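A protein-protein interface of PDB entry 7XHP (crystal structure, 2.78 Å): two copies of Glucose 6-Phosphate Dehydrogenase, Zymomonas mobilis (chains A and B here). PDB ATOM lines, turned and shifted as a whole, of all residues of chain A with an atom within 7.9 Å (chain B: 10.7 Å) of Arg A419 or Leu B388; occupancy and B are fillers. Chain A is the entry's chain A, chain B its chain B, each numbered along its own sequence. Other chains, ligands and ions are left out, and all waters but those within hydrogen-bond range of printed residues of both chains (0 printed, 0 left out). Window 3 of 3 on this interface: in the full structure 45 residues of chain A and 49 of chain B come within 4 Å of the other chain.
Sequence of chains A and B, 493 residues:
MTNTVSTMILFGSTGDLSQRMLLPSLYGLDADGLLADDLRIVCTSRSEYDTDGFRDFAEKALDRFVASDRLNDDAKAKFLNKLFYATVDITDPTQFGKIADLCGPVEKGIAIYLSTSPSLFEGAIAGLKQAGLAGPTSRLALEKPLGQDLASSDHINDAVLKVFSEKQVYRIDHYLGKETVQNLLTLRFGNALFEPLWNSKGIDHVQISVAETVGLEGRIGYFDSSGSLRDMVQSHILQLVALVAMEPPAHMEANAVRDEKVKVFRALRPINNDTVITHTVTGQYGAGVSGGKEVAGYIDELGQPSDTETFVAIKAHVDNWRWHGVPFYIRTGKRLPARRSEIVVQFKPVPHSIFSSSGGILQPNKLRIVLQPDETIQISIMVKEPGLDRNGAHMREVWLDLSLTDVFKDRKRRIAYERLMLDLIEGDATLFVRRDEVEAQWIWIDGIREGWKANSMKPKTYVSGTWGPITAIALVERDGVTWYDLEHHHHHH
N of Gly B387 is in hydrogen-bond range of OE2 of Glu A179, at 3.2 Å.
NH2 of Arg A411 sits close to O of Pro B386 (2.2 Å).
NH2 of Arg A419 lies close to N of Asp B389 (3.0 Å).
The guanidinium group (NH2) of Arg A419 sits at hydrogen-bond distance from the side-chain amide oxygen (OE1) of Gln A182.
O of Pro B386 touches CE of Lys A412, 3.6 Å away.
CA of Gly B387 touches CE of Lys A412, at 3.6 Å.
Leu B388 touches Arg A419 (CA to NE, 3.3 Å).
No residue of chain B comes within 4 Å of Gly A177.
Printed residues of chain B within 4 Å of Arg A411: Pro B386 (2.2 Å).
Of the printed residues of chain B, Lys A412 touches Pro B386 (3.6 Å) and Gly B387 (3.6 Å).
No residue of chain B comes within 4 Å of Ile A415.
No residue of chain B comes within 4 Å of Ala A416.
No residue of chain B comes within 4 Å of Glu A418.
Printed residues of chain B within 4 Å of Arg A419: Leu B388 (3.3 Å) and Asp B389 (3.0 Å).
No residue of chain B comes within 4 Å of Leu A422.
Of the printed residues of chain A, Pro B386 touches Arg A411 (2.2 Å) and Lys A412 (3.6 Å).
Gly B387 touches just these residues of chain A: Glu A179 (3.2 Å) and Lys A412 (3.6 Å).
Leu B388 touches one residue of chain A.
Printed residues of chain A within 4 Å of Asp B389: Arg A419 (3.0 Å).
The nearest residue of chain A that does not touch Leu B388 is Glu A418 (4.6 Å).
Printed residues of chain A that touch a printed residue of chain B: Glu A179, Arg A411, Lys A412 and Arg A419.
Hydrophobic or aromatic side chains of chain B that line the printed part of chain A: Pro B386 and Leu B388.
Along chain B the printed residues that touch a printed residue of chain A span positions 386 to 389.
Among the printed residues, no Asp or Glu carboxylate lies within 4 Å of a Lys or Arg side-chain nitrogen of the other chain.
No position is printed for both chains.
Of the 6 pairs that touch across the chains among the printed residues, none has its exchanged pair printed and touching as well.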
ATOM      1  N   LEU A  34     -15.258 -16.801  -4.059  1.00  0.00           N
ATOM      2  CA  LEU A  34     -14.757 -17.336  -2.773  1.00  0.00           C
ATOM      3  C   LEU A  34     -14.218 -16.131  -2.011  1.00  0.00           C
ATOM      4  O   LEU A  34     -14.599 -14.996  -2.347  1.00  0.00           O
ATOM      5  CB  LEU A  34     -13.671 -18.387  -3.022  1.00  0.00           C
ATOM      6  CG  LEU A  34     -13.716 -19.621  -2.125  1.00  0.00           C
ATOM      7  CD1 LEU A  34     -15.098 -20.255  -2.149  1.00  0.00           C
ATOM      8  CD2 LEU A  34     -12.660 -20.630  -2.548  1.00  0.00           C
ATOM      9  N   LEU A 176     -13.065 -35.096  -9.161  1.00  0.00           N
ATOM     10  CA  LEU A 176     -13.619 -35.186  -7.817  1.00  0.00           C
ATOM     11  C   LEU A 176     -14.159 -33.847  -7.333  1.00  0.00           C
ATOM     12  O   LEU A 176     -15.014 -33.816  -6.441  1.00  0.00           O
ATOM     13  CB  LEU A 176     -12.546 -35.719  -6.870  1.00  0.00           C
ATOM     14  CG  LEU A 176     -11.963 -37.048  -7.361  1.00  0.00           C
ATOM     15  CD1 LEU A 176     -10.869 -37.556  -6.439  1.00  0.00           C
ATOM     16  CD2 LEU A 176     -13.061 -38.085  -7.519  1.00  0.00           C
ATOM     17  N   GLY A 177     -13.676 -32.738  -7.899  1.00  0.00           N
ATOM     18  CA  GLY A 177     -14.179 -31.422  -7.569  1.00  0.00           C
ATOM     19  C   GLY A 177     -15.369 -30.968  -8.382  1.00  0.00           C
ATOM     20  O   GLY A 177     -15.981 -29.950  -8.051  1.00  0.00           O
ATOM     21  N   LYS A 178     -15.712 -31.692  -9.446  1.00  0.00           N
ATOM     22  CA  LYS A 178     -16.890 -31.340 -10.227  1.00  0.00           C
ATOM     23  C   LYS A 178     -18.146 -31.674  -9.436  1.00  0.00           C
ATOM     24  O   LYS A 178     -18.255 -32.757  -8.852  1.00  0.00           O
ATOM     25  CB  LYS A 178     -16.906 -32.089 -11.560  1.00  0.00           C
ATOM     26  CG  LYS A 178     -15.759 -31.785 -12.504  1.00  0.00           C
ATOM     27  CD  LYS A 178     -15.606 -32.903 -13.526  1.00  0.00           C
ATOM     28  CE  LYS A 178     -14.985 -32.405 -14.817  1.00  0.00           C
ATOM     29  NZ  LYS A 178     -15.134 -30.931 -14.964  1.00  0.00           N
ATOM     30  N   GLU A 179     -19.093 -30.736  -9.407  1.00  0.00           N
ATOM     31  CA  GLU A 179     -20.325 -30.956  -8.656  1.00  0.00           C
ATOM     32  C   GLU A 179     -21.081 -32.156  -9.209  1.00  0.00           C
ATOM     33  O   GLU A 179     -21.556 -33.013  -8.457  1.00  0.00           O
ATOM     34  CB  GLU A 179     -21.205 -29.711  -8.726  1.00  0.00           C
ATOM     35  CG  GLU A 179     -20.459 -28.404  -8.578  1.00  0.00           C
ATOM     36  CD  GLU A 179     -21.070 -27.509  -7.531  1.00  0.00           C
ATOM     37  OE1 GLU A 179     -21.368 -26.340  -7.853  1.00  0.00           O
ATOM     38  OE2 GLU A 179     -21.241 -27.969  -6.383  1.00  0.00           O
ATOM     39  N   GLN A 182     -19.813 -35.169  -7.839  1.00  0.00           N
ATOM     40  CA  GLN A 182     -20.049 -35.290  -6.404  1.00  0.00           C
ATOM     41  C   GLN A 182     -21.396 -35.926  -6.087  1.00  0.00           C
ATOM     42  O   GLN A 182     -21.516 -36.665  -5.102  1.00  0.00           O
ATOM     43  CB  GLN A 182     -20.009 -33.904  -5.760  1.00  0.00           C
ATOM     44  CG  GLN A 182     -18.658 -33.376  -5.358  1.00  0.00           C
ATOM     45  CD  GLN A 182     -18.745 -31.933  -4.912  1.00  0.00           C
ATOM     46  OE1 GLN A 182     -19.187 -31.636  -3.801  1.00  0.00           O
ATOM     47  NE2 GLN A 182     -18.345 -31.021  -5.788  1.00  0.00           N
ATOM     48  N   ARG A 411     -28.921 -20.866  -9.279  1.00  0.00           N
ATOM     49  CA  ARG A 411     -27.865 -21.322  -8.396  1.00  0.00           C
ATOM     50  C   ARG A 411     -26.503 -21.101  -9.039  1.00  0.00           C
ATOM     51  O   ARG A 411     -26.384 -20.590 -10.155  1.00  0.00           O
ATOM     52  CB  ARG A 411     -28.062 -22.798  -8.040  1.00  0.00           C
ATOM     53  CG  ARG A 411     -29.349 -23.086  -7.292  1.00  0.00           C
ATOM     54  CD  ARG A 411     -29.285 -22.474  -5.949  1.00  0.00           C
ATOM     55  NE  ARG A 411     -28.344 -23.246  -5.162  1.00  0.00           N
ATOM     56  CZ  ARG A 411     -27.291 -22.739  -4.545  1.00  0.00           C
ATOM     57  NH1 ARG A 411     -26.999 -21.451  -4.619  1.00  0.00           N
ATOM     58  NH2 ARG A 411     -26.504 -23.548  -3.844  1.00  0.00           N
ATOM     59  N   LYS A 412     -25.457 -21.512  -8.335  1.00  0.00           N
ATOM     60  CA  LYS A 412     -24.123 -21.123  -8.745  1.00  0.00           C
ATOM     61  C   LYS A 412     -23.518 -22.138  -9.706  1.00  0.00           C
ATOM     62  O   LYS A 412     -23.945 -23.290  -9.801  1.00  0.00           O
ATOM     63  CB  LYS A 412     -23.221 -20.970  -7.518  1.00  0.00           C
ATOM     64  CG  LYS A 412     -23.322 -22.129  -6.528  1.00  0.00           C
ATOM     65  CD  LYS A 412     -22.569 -21.846  -5.234  1.00  0.00           C
ATOM     66  CE  LYS A 412     -23.278 -22.455  -4.031  1.00  0.00           C
ATOM     67  NZ  LYS A 412     -24.115 -21.456  -3.308  1.00  0.00           N
ATOM     68  N   ARG A 414     -20.083 -22.868  -9.491  1.00  0.00           N
ATOM     69  CA  ARG A 414     -18.750 -22.745  -8.856  1.00  0.00           C
ATOM     70  C   ARG A 414     -17.742 -23.678  -9.518  1.00  0.00           C
ATOM     71  O   ARG A 414     -18.109 -24.821  -9.834  1.00  0.00           O
ATOM     72  CB  ARG A 414     -18.857 -23.060  -7.362  1.00  0.00           C
ATOM     73  N   ILE A 415     -16.510 -23.201  -9.685  1.00  0.00           N
ATOM     74  CA  ILE A 415     -15.421 -24.031 -10.273  1.00  0.00           C
ATOM     75  C   ILE A 415     -15.018 -25.114  -9.269  1.00  0.00           C
ATOM     76  O   ILE A 415     -15.182 -24.891  -8.057  1.00  0.00           O
ATOM     77  CB  ILE A 415     -14.227 -23.148 -10.687  1.00  0.00           C
ATOM     78  N   ALA A 416     -14.492 -26.234  -9.762  1.00  0.00           N
ATOM     79  CA  ALA A 416     -14.102 -27.363  -8.892  1.00  0.00           C
ATOM     80  C   ALA A 416     -13.019 -26.872  -7.945  1.00  0.00           C
ATOM     81  O   ALA A 416     -13.064 -27.208  -6.754  1.00  0.00           O
ATOM     82  CB  ALA A 416     -13.569 -28.471  -9.754  1.00  0.00           C
ATOM     83  N   TYR A 417     -12.110 -26.058  -8.465  1.00  0.00           N
ATOM     84  CA  TYR A 417     -10.984 -25.552  -7.650  1.00  0.00           C
ATOM     85  C   TYR A 417     -11.565 -24.720  -6.504  1.00  0.00           C
ATOM     86  O   TYR A 417     -11.028 -24.829  -5.396  1.00  0.00           O
ATOM     87  CB  TYR A 417      -9.960 -24.892  -8.575  1.00  0.00           C
ATOM     88  CG  TYR A 417      -9.357 -25.903  -9.513  1.00  0.00           C
ATOM     89  CD1 TYR A 417      -8.302 -26.703  -9.114  1.00  0.00           C
ATOM     90  CD2 TYR A 417      -9.894 -26.119 -10.771  1.00  0.00           C
ATOM     91  CE1 TYR A 417      -7.763 -27.660  -9.956  1.00  0.00           C
ATOM     92  CE2 TYR A 417      -9.367 -27.072 -11.626  1.00  0.00           C
ATOM     93  CZ  TYR A 417      -8.297 -27.846 -11.216  1.00  0.00           C
ATOM     94  OH  TYR A 417      -7.772 -28.786 -12.054  1.00  0.00           O
ATOM     95  N   GLU A 418     -12.619 -23.943  -6.734  1.00  0.00           N
ATOM     96  CA  GLU A 418     -13.147 -23.191  -5.571  1.00  0.00           C
ATOM     97  C   GLU A 418     -13.644 -24.131  -4.461  1.00  0.00           C
ATOM     98  O   GLU A 418     -13.342 -23.844  -3.293  1.00  0.00           O
ATOM     99  CB  GLU A 418     -14.324 -22.323  -6.012  1.00  0.00           C
ATOM    100  CG  GLU A 418     -14.183 -21.766  -7.414  1.00  0.00           C
ATOM    101  CD  GLU A 418     -15.276 -20.787  -7.806  1.00  0.00           C
ATOM    102  OE1 GLU A 418     -15.730 -20.842  -8.961  1.00  0.00           O
ATOM    103  OE2 GLU A 418     -15.669 -19.971  -6.952  1.00  0.00           O
ATOM    104  N   ARG A 419     -14.380 -25.197  -4.780  1.00  0.00           N
ATOM    105  CA  ARG A 419     -14.777 -26.165  -3.719  1.00  0.00           C
ATOM    106  C   ARG A 419     -13.559 -26.877  -3.132  1.00  0.00           C
ATOM    107  O   ARG A 419     -13.475 -26.988  -1.899  1.00  0.00           O
ATOM    108  CB  ARG A 419     -15.742 -27.204  -4.297  1.00  0.00           C
ATOM    109  CG  ARG A 419     -15.835 -28.496  -3.500  1.00  0.00           C
ATOM    110  CD  ARG A 419     -16.645 -28.309  -2.234  1.00  0.00           C
ATOM    111  NE  ARG A 419     -17.750 -29.249  -2.117  1.00  0.00           N
ATOM    112  CZ  ARG A 419     -17.761 -30.293  -1.297  1.00  0.00           C
ATOM    113  NH1 ARG A 419     -16.720 -30.536  -0.521  1.00  0.00           N
ATOM    114  NH2 ARG A 419     -18.812 -31.090  -1.258  1.00  0.00           N
ATOM    115  N   LEU A 420     -12.636 -27.299  -3.990  1.00  0.00           N
ATOM    116  CA  LEU A 420     -11.447 -28.082  -3.560  1.00  0.00           C
ATOM    117  C   LEU A 420     -10.548 -27.250  -2.650  1.00  0.00           C
ATOM    118  O   LEU A 420      -9.993 -27.813  -1.699  1.00  0.00           O
ATOM    119  CB  LEU A 420     -10.711 -28.561  -4.815  1.00  0.00           C
ATOM    120  CG  LEU A 420     -11.487 -29.538  -5.696  1.00  0.00           C
ATOM    121  CD1 LEU A 420     -10.878 -29.613  -7.087  1.00  0.00           C
ATOM    122  CD2 LEU A 420     -11.534 -30.915  -5.062  1.00  0.00           C
ATOM    123  N   MET A 421     -10.402 -25.963  -2.947  1.00  0.00           N
ATOM    124  CA  MET A 421      -9.425 -25.125  -2.209  1.00  0.00           C
ATOM    125  C   MET A 421      -9.748 -25.038  -0.712  1.00  0.00           C
ATOM    126  O   MET A 421      -8.797 -25.134   0.076  1.00  0.00           O
ATOM    127  CB  MET A 421      -9.433 -23.720  -2.816  1.00  0.00           C
ATOM    128  CG  MET A 421      -8.593 -23.613  -4.069  1.00  0.00           C
ATOM    129  SD  MET A 421      -8.078 -25.242  -4.663  1.00  0.00           S
ATOM    130  CE  MET A 421      -6.378 -25.278  -4.100  1.00  0.00           C
ATOM    131  N   LEU A 422     -11.016 -24.893  -0.325  1.00  0.00           N
ATOM    132  CA  LEU A 422     -11.348 -24.714   1.116  1.00  0.00           C
ATOM    133  C   LEU A 422     -10.920 -25.967   1.876  1.00  0.00           C
ATOM    134  O   LEU A 422     -10.332 -25.820   2.955  1.00  0.00           O
ATOM    135  CB  LEU A 422     -12.849 -24.461   1.255  1.00  0.00           C
ATOM    136  N   ASP A 423     -11.233 -27.148   1.346  1.00  0.00           N
ATOM    137  CA  ASP A 423     -10.811 -28.410   1.944  1.00  0.00           C
ATOM    138  C   ASP A 423      -9.310 -28.431   2.214  1.00  0.00           C
ATOM    139  O   ASP A 423      -8.871 -28.891   3.274  1.00  0.00           O
ATOM    140  CB  ASP A 423     -11.203 -29.562   1.018  1.00  0.00           C
ATOM    141  CG  ASP A 423     -12.577 -30.122   1.327  1.00  0.00           C
ATOM    142  OD1 ASP A 423     -13.509 -29.327   1.565  1.00  0.00           O
ATOM    143  OD2 ASP A 423     -12.722 -31.364   1.332  1.00  0.00           O
ATOM    144  N   LEU A 424      -8.505 -27.910   1.292  1.00  0.00           N
ATOM    145  CA  LEU A 424      -7.046 -27.832   1.568  1.00  0.00           C
ATOM    146  C   LEU A 424      -6.836 -27.048   2.865  1.00  0.00           C
ATOM    147  O   LEU A 424      -6.103 -27.542   3.734  1.00  0.00           O
ATOM    148  CB  LEU A 424      -6.341 -27.152   0.392  1.00  0.00           C
ATOM    149  CG  LEU A 424      -4.816 -27.163   0.441  1.00  0.00           C
ATOM    150  CD1 LEU A 424      -4.275 -28.558   0.181  1.00  0.00           C
ATOM    151  CD2 LEU A 424      -4.244 -26.176  -0.562  1.00  0.00           C
ATOM    152  N   ILE A 425      -7.436 -25.862   2.970  1.00  0.00           N
ATOM    153  CA  ILE A 425      -7.350 -25.031   4.208  1.00  0.00           C
ATOM    154  C   ILE A 425      -8.012 -25.767   5.380  1.00  0.00           C
ATOM    155  O   ILE A 425      -7.441 -25.732   6.483  1.00  0.00           O
ATOM    156  CB  ILE A 425      -7.984 -23.648   3.960  1.00  0.00           C
ATOM    157  CG1 ILE A 425      -7.328 -22.935   2.777  1.00  0.00           C
ATOM    158  CG2 ILE A 425      -7.950 -22.800   5.221  1.00  0.00           C
ATOM    159  CD1 ILE A 425      -8.309 -22.338   1.797  1.00  0.00           C
ATOM    160  N   ALA A 429      -9.649 -32.953   4.714  1.00  0.00           N
ATOM    161  CA  ALA A 429     -10.209 -32.711   3.370  1.00  0.00           C
ATOM    162  C   ALA A 429     -10.667 -34.037   2.783  1.00  0.00           C
ATOM    163  O   ALA A 429     -10.037 -35.061   3.082  1.00  0.00           O
ATOM    164  CB  ALA A 429      -9.212 -32.018   2.492  1.00  0.00           C
ATOM    165  N   THR A 430     -11.733 -34.000   1.992  1.00  0.00           N
ATOM    166  CA  THR A 430     -12.328 -35.211   1.437  1.00  0.00           C
ATOM    167  C   THR A 430     -12.073 -35.465  -0.046  1.00  0.00           C
ATOM    168  O   THR A 430     -12.155 -36.621  -0.475  1.00  0.00           O
ATOM    169  CB  THR A 430     -13.848 -35.148   1.628  1.00  0.00           C
ATOM    170  OG1 THR A 430     -14.284 -33.796   1.445  1.00  0.00           O
ATOM    171  CG2 THR A 430     -14.236 -35.580   3.017  1.00  0.00           C
ATOM    172  N   LEU A 431     -11.758 -34.443  -0.842  1.00  0.00           N
ATOM    173  CA  LEU A 431     -11.712 -34.578  -2.295  1.00  0.00           C
ATOM    174  C   LEU A 431     -10.298 -34.691  -2.856  1.00  0.00           C
ATOM    175  O   LEU A 431     -10.030 -34.209  -3.964  1.00  0.00           O
ATOM    176  CB  LEU A 431     -12.459 -33.420  -2.944  1.00  0.00           C
ATOM    177  CG  LEU A 431     -13.783 -33.090  -2.253  1.00  0.00           C
ATOM    178  CD1 LEU A 431     -14.357 -31.795  -2.797  1.00  0.00           C
ATOM    179  CD2 LEU A 431     -14.781 -34.237  -2.398  1.00  0.00           C
ATOM    180  N   PHE A 432      -9.394 -35.332  -2.131  1.00  0.00           N
ATOM    181  CA  PHE A 432      -8.004 -35.421  -2.540  1.00  0.00           C
ATOM    182  C   PHE A 432      -7.560 -36.874  -2.517  1.00  0.00           C
ATOM    183  O   PHE A 432      -8.002 -37.652  -1.673  1.00  0.00           O
ATOM    184  CB  PHE A 432      -7.135 -34.550  -1.635  1.00  0.00           C
ATOM    185  CG  PHE A 432      -7.465 -33.084  -1.726  1.00  0.00           C
ATOM    186  CD1 PHE A 432      -6.847 -32.275  -2.662  1.00  0.00           C
ATOM    187  CD2 PHE A 432      -8.425 -32.523  -0.899  1.00  0.00           C
ATOM    188  CE1 PHE A 432      -7.158 -30.929  -2.753  1.00  0.00           C
ATOM    189  CE2 PHE A 432      -8.742 -31.179  -0.988  1.00  0.00           C
ATOM    190  CZ  PHE A 432      -8.108 -30.383  -1.914  1.00  0.00           C
ATOM    191  N   PHE B 355     -25.823 -39.573   5.643  1.00  0.00           N
ATOM    192  CA  PHE B 355     -25.661 -38.102   5.686  1.00  0.00           C
ATOM    193  C   PHE B 355     -26.144 -37.678   7.068  1.00  0.00           C
ATOM    194  O   PHE B 355     -26.969 -36.757   7.165  1.00  0.00           O
ATOM    195  CB  PHE B 355     -26.424 -37.484   4.514  1.00  0.00           C
ATOM    196  CG  PHE B 355     -26.363 -38.308   3.254  1.00  0.00           C
ATOM    197  CD1 PHE B 355     -25.392 -38.069   2.295  1.00  0.00           C
ATOM    198  CD2 PHE B 355     -27.261 -39.339   3.034  1.00  0.00           C
ATOM    199  CE1 PHE B 355     -25.329 -38.833   1.142  1.00  0.00           C
ATOM    200  CE2 PHE B 355     -27.193 -40.106   1.883  1.00  0.00           C
ATOM    201  CZ  PHE B 355     -26.229 -39.850   0.937  1.00  0.00           C
ATOM    202  N   SER B 358     -26.735 -34.336  10.918  1.00  0.00           N
ATOM    203  CA  SER B 358     -27.627 -33.210  10.533  1.00  0.00           C
ATOM    204  C   SER B 358     -27.335 -32.720   9.111  1.00  0.00           C
ATOM    205  O   SER B 358     -26.277 -33.074   8.562  1.00  0.00           O
ATOM    206  CB  SER B 358     -27.607 -32.072  11.527  1.00  0.00           C
ATOM    207  OG  SER B 358     -28.385 -32.390  12.668  1.00  0.00           O
ATOM    208  N   GLY B 359     -28.258 -31.951   8.542  1.00  0.00           N
ATOM    209  CA  GLY B 359     -28.086 -31.335   7.214  1.00  0.00           C
ATOM    210  C   GLY B 359     -28.547 -32.217   6.076  1.00  0.00           C
ATOM    211  O   GLY B 359     -28.741 -31.673   4.982  1.00  0.00           O
ATOM    212  N   LYS B 384     -28.061 -33.902  -4.363  1.00  0.00           N
ATOM    213  CA  LYS B 384     -27.294 -32.876  -3.674  1.00  0.00           C
ATOM    214  C   LYS B 384     -27.622 -31.502  -4.247  1.00  0.00           C
ATOM    215  O   LYS B 384     -27.827 -31.345  -5.453  1.00  0.00           O
ATOM    216  CB  LYS B 384     -25.795 -33.160  -3.793  1.00  0.00           C
ATOM    217  N   GLU B 385     -27.703 -30.518  -3.373  1.00  0.00           N
ATOM    218  CA  GLU B 385     -27.973 -29.148  -3.786  1.00  0.00           C
ATOM    219  C   GLU B 385     -26.673 -28.504  -4.260  1.00  0.00           C
ATOM    220  O   GLU B 385     -25.635 -28.677  -3.615  1.00  0.00           O
ATOM    221  CB  GLU B 385     -28.547 -28.347  -2.615  1.00  0.00           C
ATOM    222  CG  GLU B 385     -29.384 -27.141  -3.007  1.00  0.00           C
ATOM    223  CD  GLU B 385     -30.868 -27.402  -2.888  1.00  0.00           C
ATOM    224  OE1 GLU B 385     -31.232 -28.535  -2.517  1.00  0.00           O
ATOM    225  OE2 GLU B 385     -31.666 -26.479  -3.157  1.00  0.00           O
ATOM    226  N   PRO B 386     -26.683 -27.793  -5.390  1.00  0.00           N
ATOM    227  CA  PRO B 386     -25.418 -27.271  -5.932  1.00  0.00           C
ATOM    228  C   PRO B 386     -24.774 -26.336  -4.923  1.00  0.00           C
ATOM    229  O   PRO B 386     -25.342 -25.309  -4.547  1.00  0.00           O
ATOM    230  CB  PRO B 386     -25.856 -26.536  -7.203  1.00  0.00           C
ATOM    231  CG  PRO B 386     -27.288 -26.200  -6.982  1.00  0.00           C
ATOM    232  CD  PRO B 386     -27.855 -27.284  -6.121  1.00  0.00           C
ATOM    233  N   GLY B 387     -23.560 -26.674  -4.530  1.00  0.00           N
ATOM    234  CA  GLY B 387     -22.911 -26.012  -3.420  1.00  0.00           C
ATOM    235  C   GLY B 387     -21.938 -26.974  -2.772  1.00  0.00           C
ATOM    236  O   GLY B 387     -21.741 -28.094  -3.240  1.00  0.00           O
ATOM    237  N   LEU B 388     -21.271 -26.501  -1.715  1.00  0.00           N
ATOM    238  CA  LEU B 388     -20.209 -27.306  -1.059  1.00  0.00           C
ATOM    239  C   LEU B 388     -20.773 -28.055   0.150  1.00  0.00           C
ATOM    240  O   LEU B 388     -21.835 -27.650   0.652  1.00  0.00           O
ATOM    241  CB  LEU B 388     -19.098 -26.345  -0.630  1.00  0.00           C
ATOM    242  CG  LEU B 388     -19.052 -25.017  -1.380  1.00  0.00           C
ATOM    243  CD1 LEU B 388     -19.449 -23.869  -0.469  1.00  0.00           C
ATOM    244  CD2 LEU B 388     -17.670 -24.775  -1.966  1.00  0.00           C
ATOM    245  N   ASP B 389     -20.066 -29.094   0.602  1.00  0.00           N
ATOM    246  CA  ASP B 389     -20.572 -29.899   1.740  1.00  0.00           C
ATOM    247  C   ASP B 389     -20.663 -28.983   2.959  1.00  0.00           C
ATOM    248  O   ASP B 389     -21.679 -29.054   3.663  1.00  0.00           O
ATOM    249  CB  ASP B 389     -19.689 -31.119   2.004  1.00  0.00           C
ATOM    250  CG  ASP B 389     -20.106 -31.920   3.221  1.00  0.00           C
ATOM    251  OD1 ASP B 389     -19.835 -31.459   4.344  1.00  0.00           O
ATOM    252  OD2 ASP B 389     -20.694 -33.001   3.035  1.00  0.00           O
ATOM    253  N   ARG B 390     -19.665 -28.125   3.179  1.00  0.00           N
ATOM    254  CA  ARG B 390     -19.806 -27.139   4.283  1.00  0.00           C
ATOM    255  C   ARG B 390     -20.068 -27.929   5.559  1.00  0.00           C
ATOM    256  O   ARG B 390     -19.296 -28.862   5.847  1.00  0.00           O
ATOM    257  CB  ARG B 390     -20.943 -26.153   3.998  1.00  0.00           C
ATOM    258  N   ASN B 391     -21.123 -27.565   6.288  1.00  0.00           N
ATOM    259  CA  ASN B 391     -21.487 -28.391   7.460  1.00  0.00           C
ATOM    260  C   ASN B 391     -22.653 -29.280   7.041  1.00  0.00           C
ATOM    261  O   ASN B 391     -23.715 -28.735   6.707  1.00  0.00           O
ATOM    262  CB  ASN B 391     -21.873 -27.528   8.661  1.00  0.00           C
ATOM    263  N   GLY B 392     -22.459 -30.598   7.103  1.00  0.00           N
ATOM    264  CA  GLY B 392     -23.507 -31.558   6.705  1.00  0.00           C
ATOM    265  C   GLY B 392     -23.544 -31.792   5.205  1.00  0.00           C
ATOM    266  O   GLY B 392     -22.730 -31.188   4.496  1.00  0.00           O
ATOM    267  N   ALA B 393     -24.464 -32.637   4.737  1.00  0.00           N
ATOM    268  CA  ALA B 393     -24.646 -32.853   3.287  1.00  0.00           C
ATOM    269  C   ALA B 393     -26.030 -32.316   2.947  1.00  0.00           C
ATOM    270  O   ALA B 393     -27.001 -32.791   3.553  1.00  0.00           O
ATOM    271  CB  ALA B 393     -24.518 -34.315   2.964  1.00  0.00           C
ATOM    272  N   HIS B 394     -26.118 -31.357   2.029  1.00  0.00           N
ATOM    273  CA  HIS B 394     -27.406 -30.736   1.779  1.00  0.00           C
ATOM    274  C   HIS B 394     -27.963 -31.283   0.476  1.00  0.00           C
ATOM    275  O   HIS B 394     -27.232 -31.450  -0.506  1.00  0.00           O
ATOM    276  CB  HIS B 394     -27.265 -29.211   1.741  1.00  0.00           C
ATOM    277  CG  HIS B 394     -26.520 -28.654   2.917  1.00  0.00           C
ATOM    278  ND1 HIS B 394     -25.154 -28.472   2.922  1.00  0.00           N
ATOM    279  CD2 HIS B 394     -26.956 -28.255   4.135  1.00  0.00           C
ATOM    280  CE1 HIS B 394     -24.782 -27.972   4.087  1.00  0.00           C
ATOM    281  NE2 HIS B 394     -25.857 -27.831   4.842  1.00  0.00           N
ATOM    282  N   MET B 395     -29.267 -31.538   0.469  1.00  0.00           N
ATOM    283  CA  MET B 395     -29.896 -32.230  -0.640  1.00  0.00           C
ATOM    284  C   MET B 395     -31.289 -31.676  -0.878  1.00  0.00           C
ATOM    285  O   MET B 395     -31.857 -30.968  -0.043  1.00  0.00           O
ATOM    286  CB  MET B 395     -30.002 -33.739  -0.360  1.00  0.00           C
ATOM    287  CG  MET B 395     -28.690 -34.428  -0.007  1.00  0.00           C
ATOM    288  SD  MET B 395     -28.811 -35.416   1.503  1.00  0.00           S
ATOM    289  CE  MET B 395     -29.889 -36.752   0.994  1.00  0.00           C
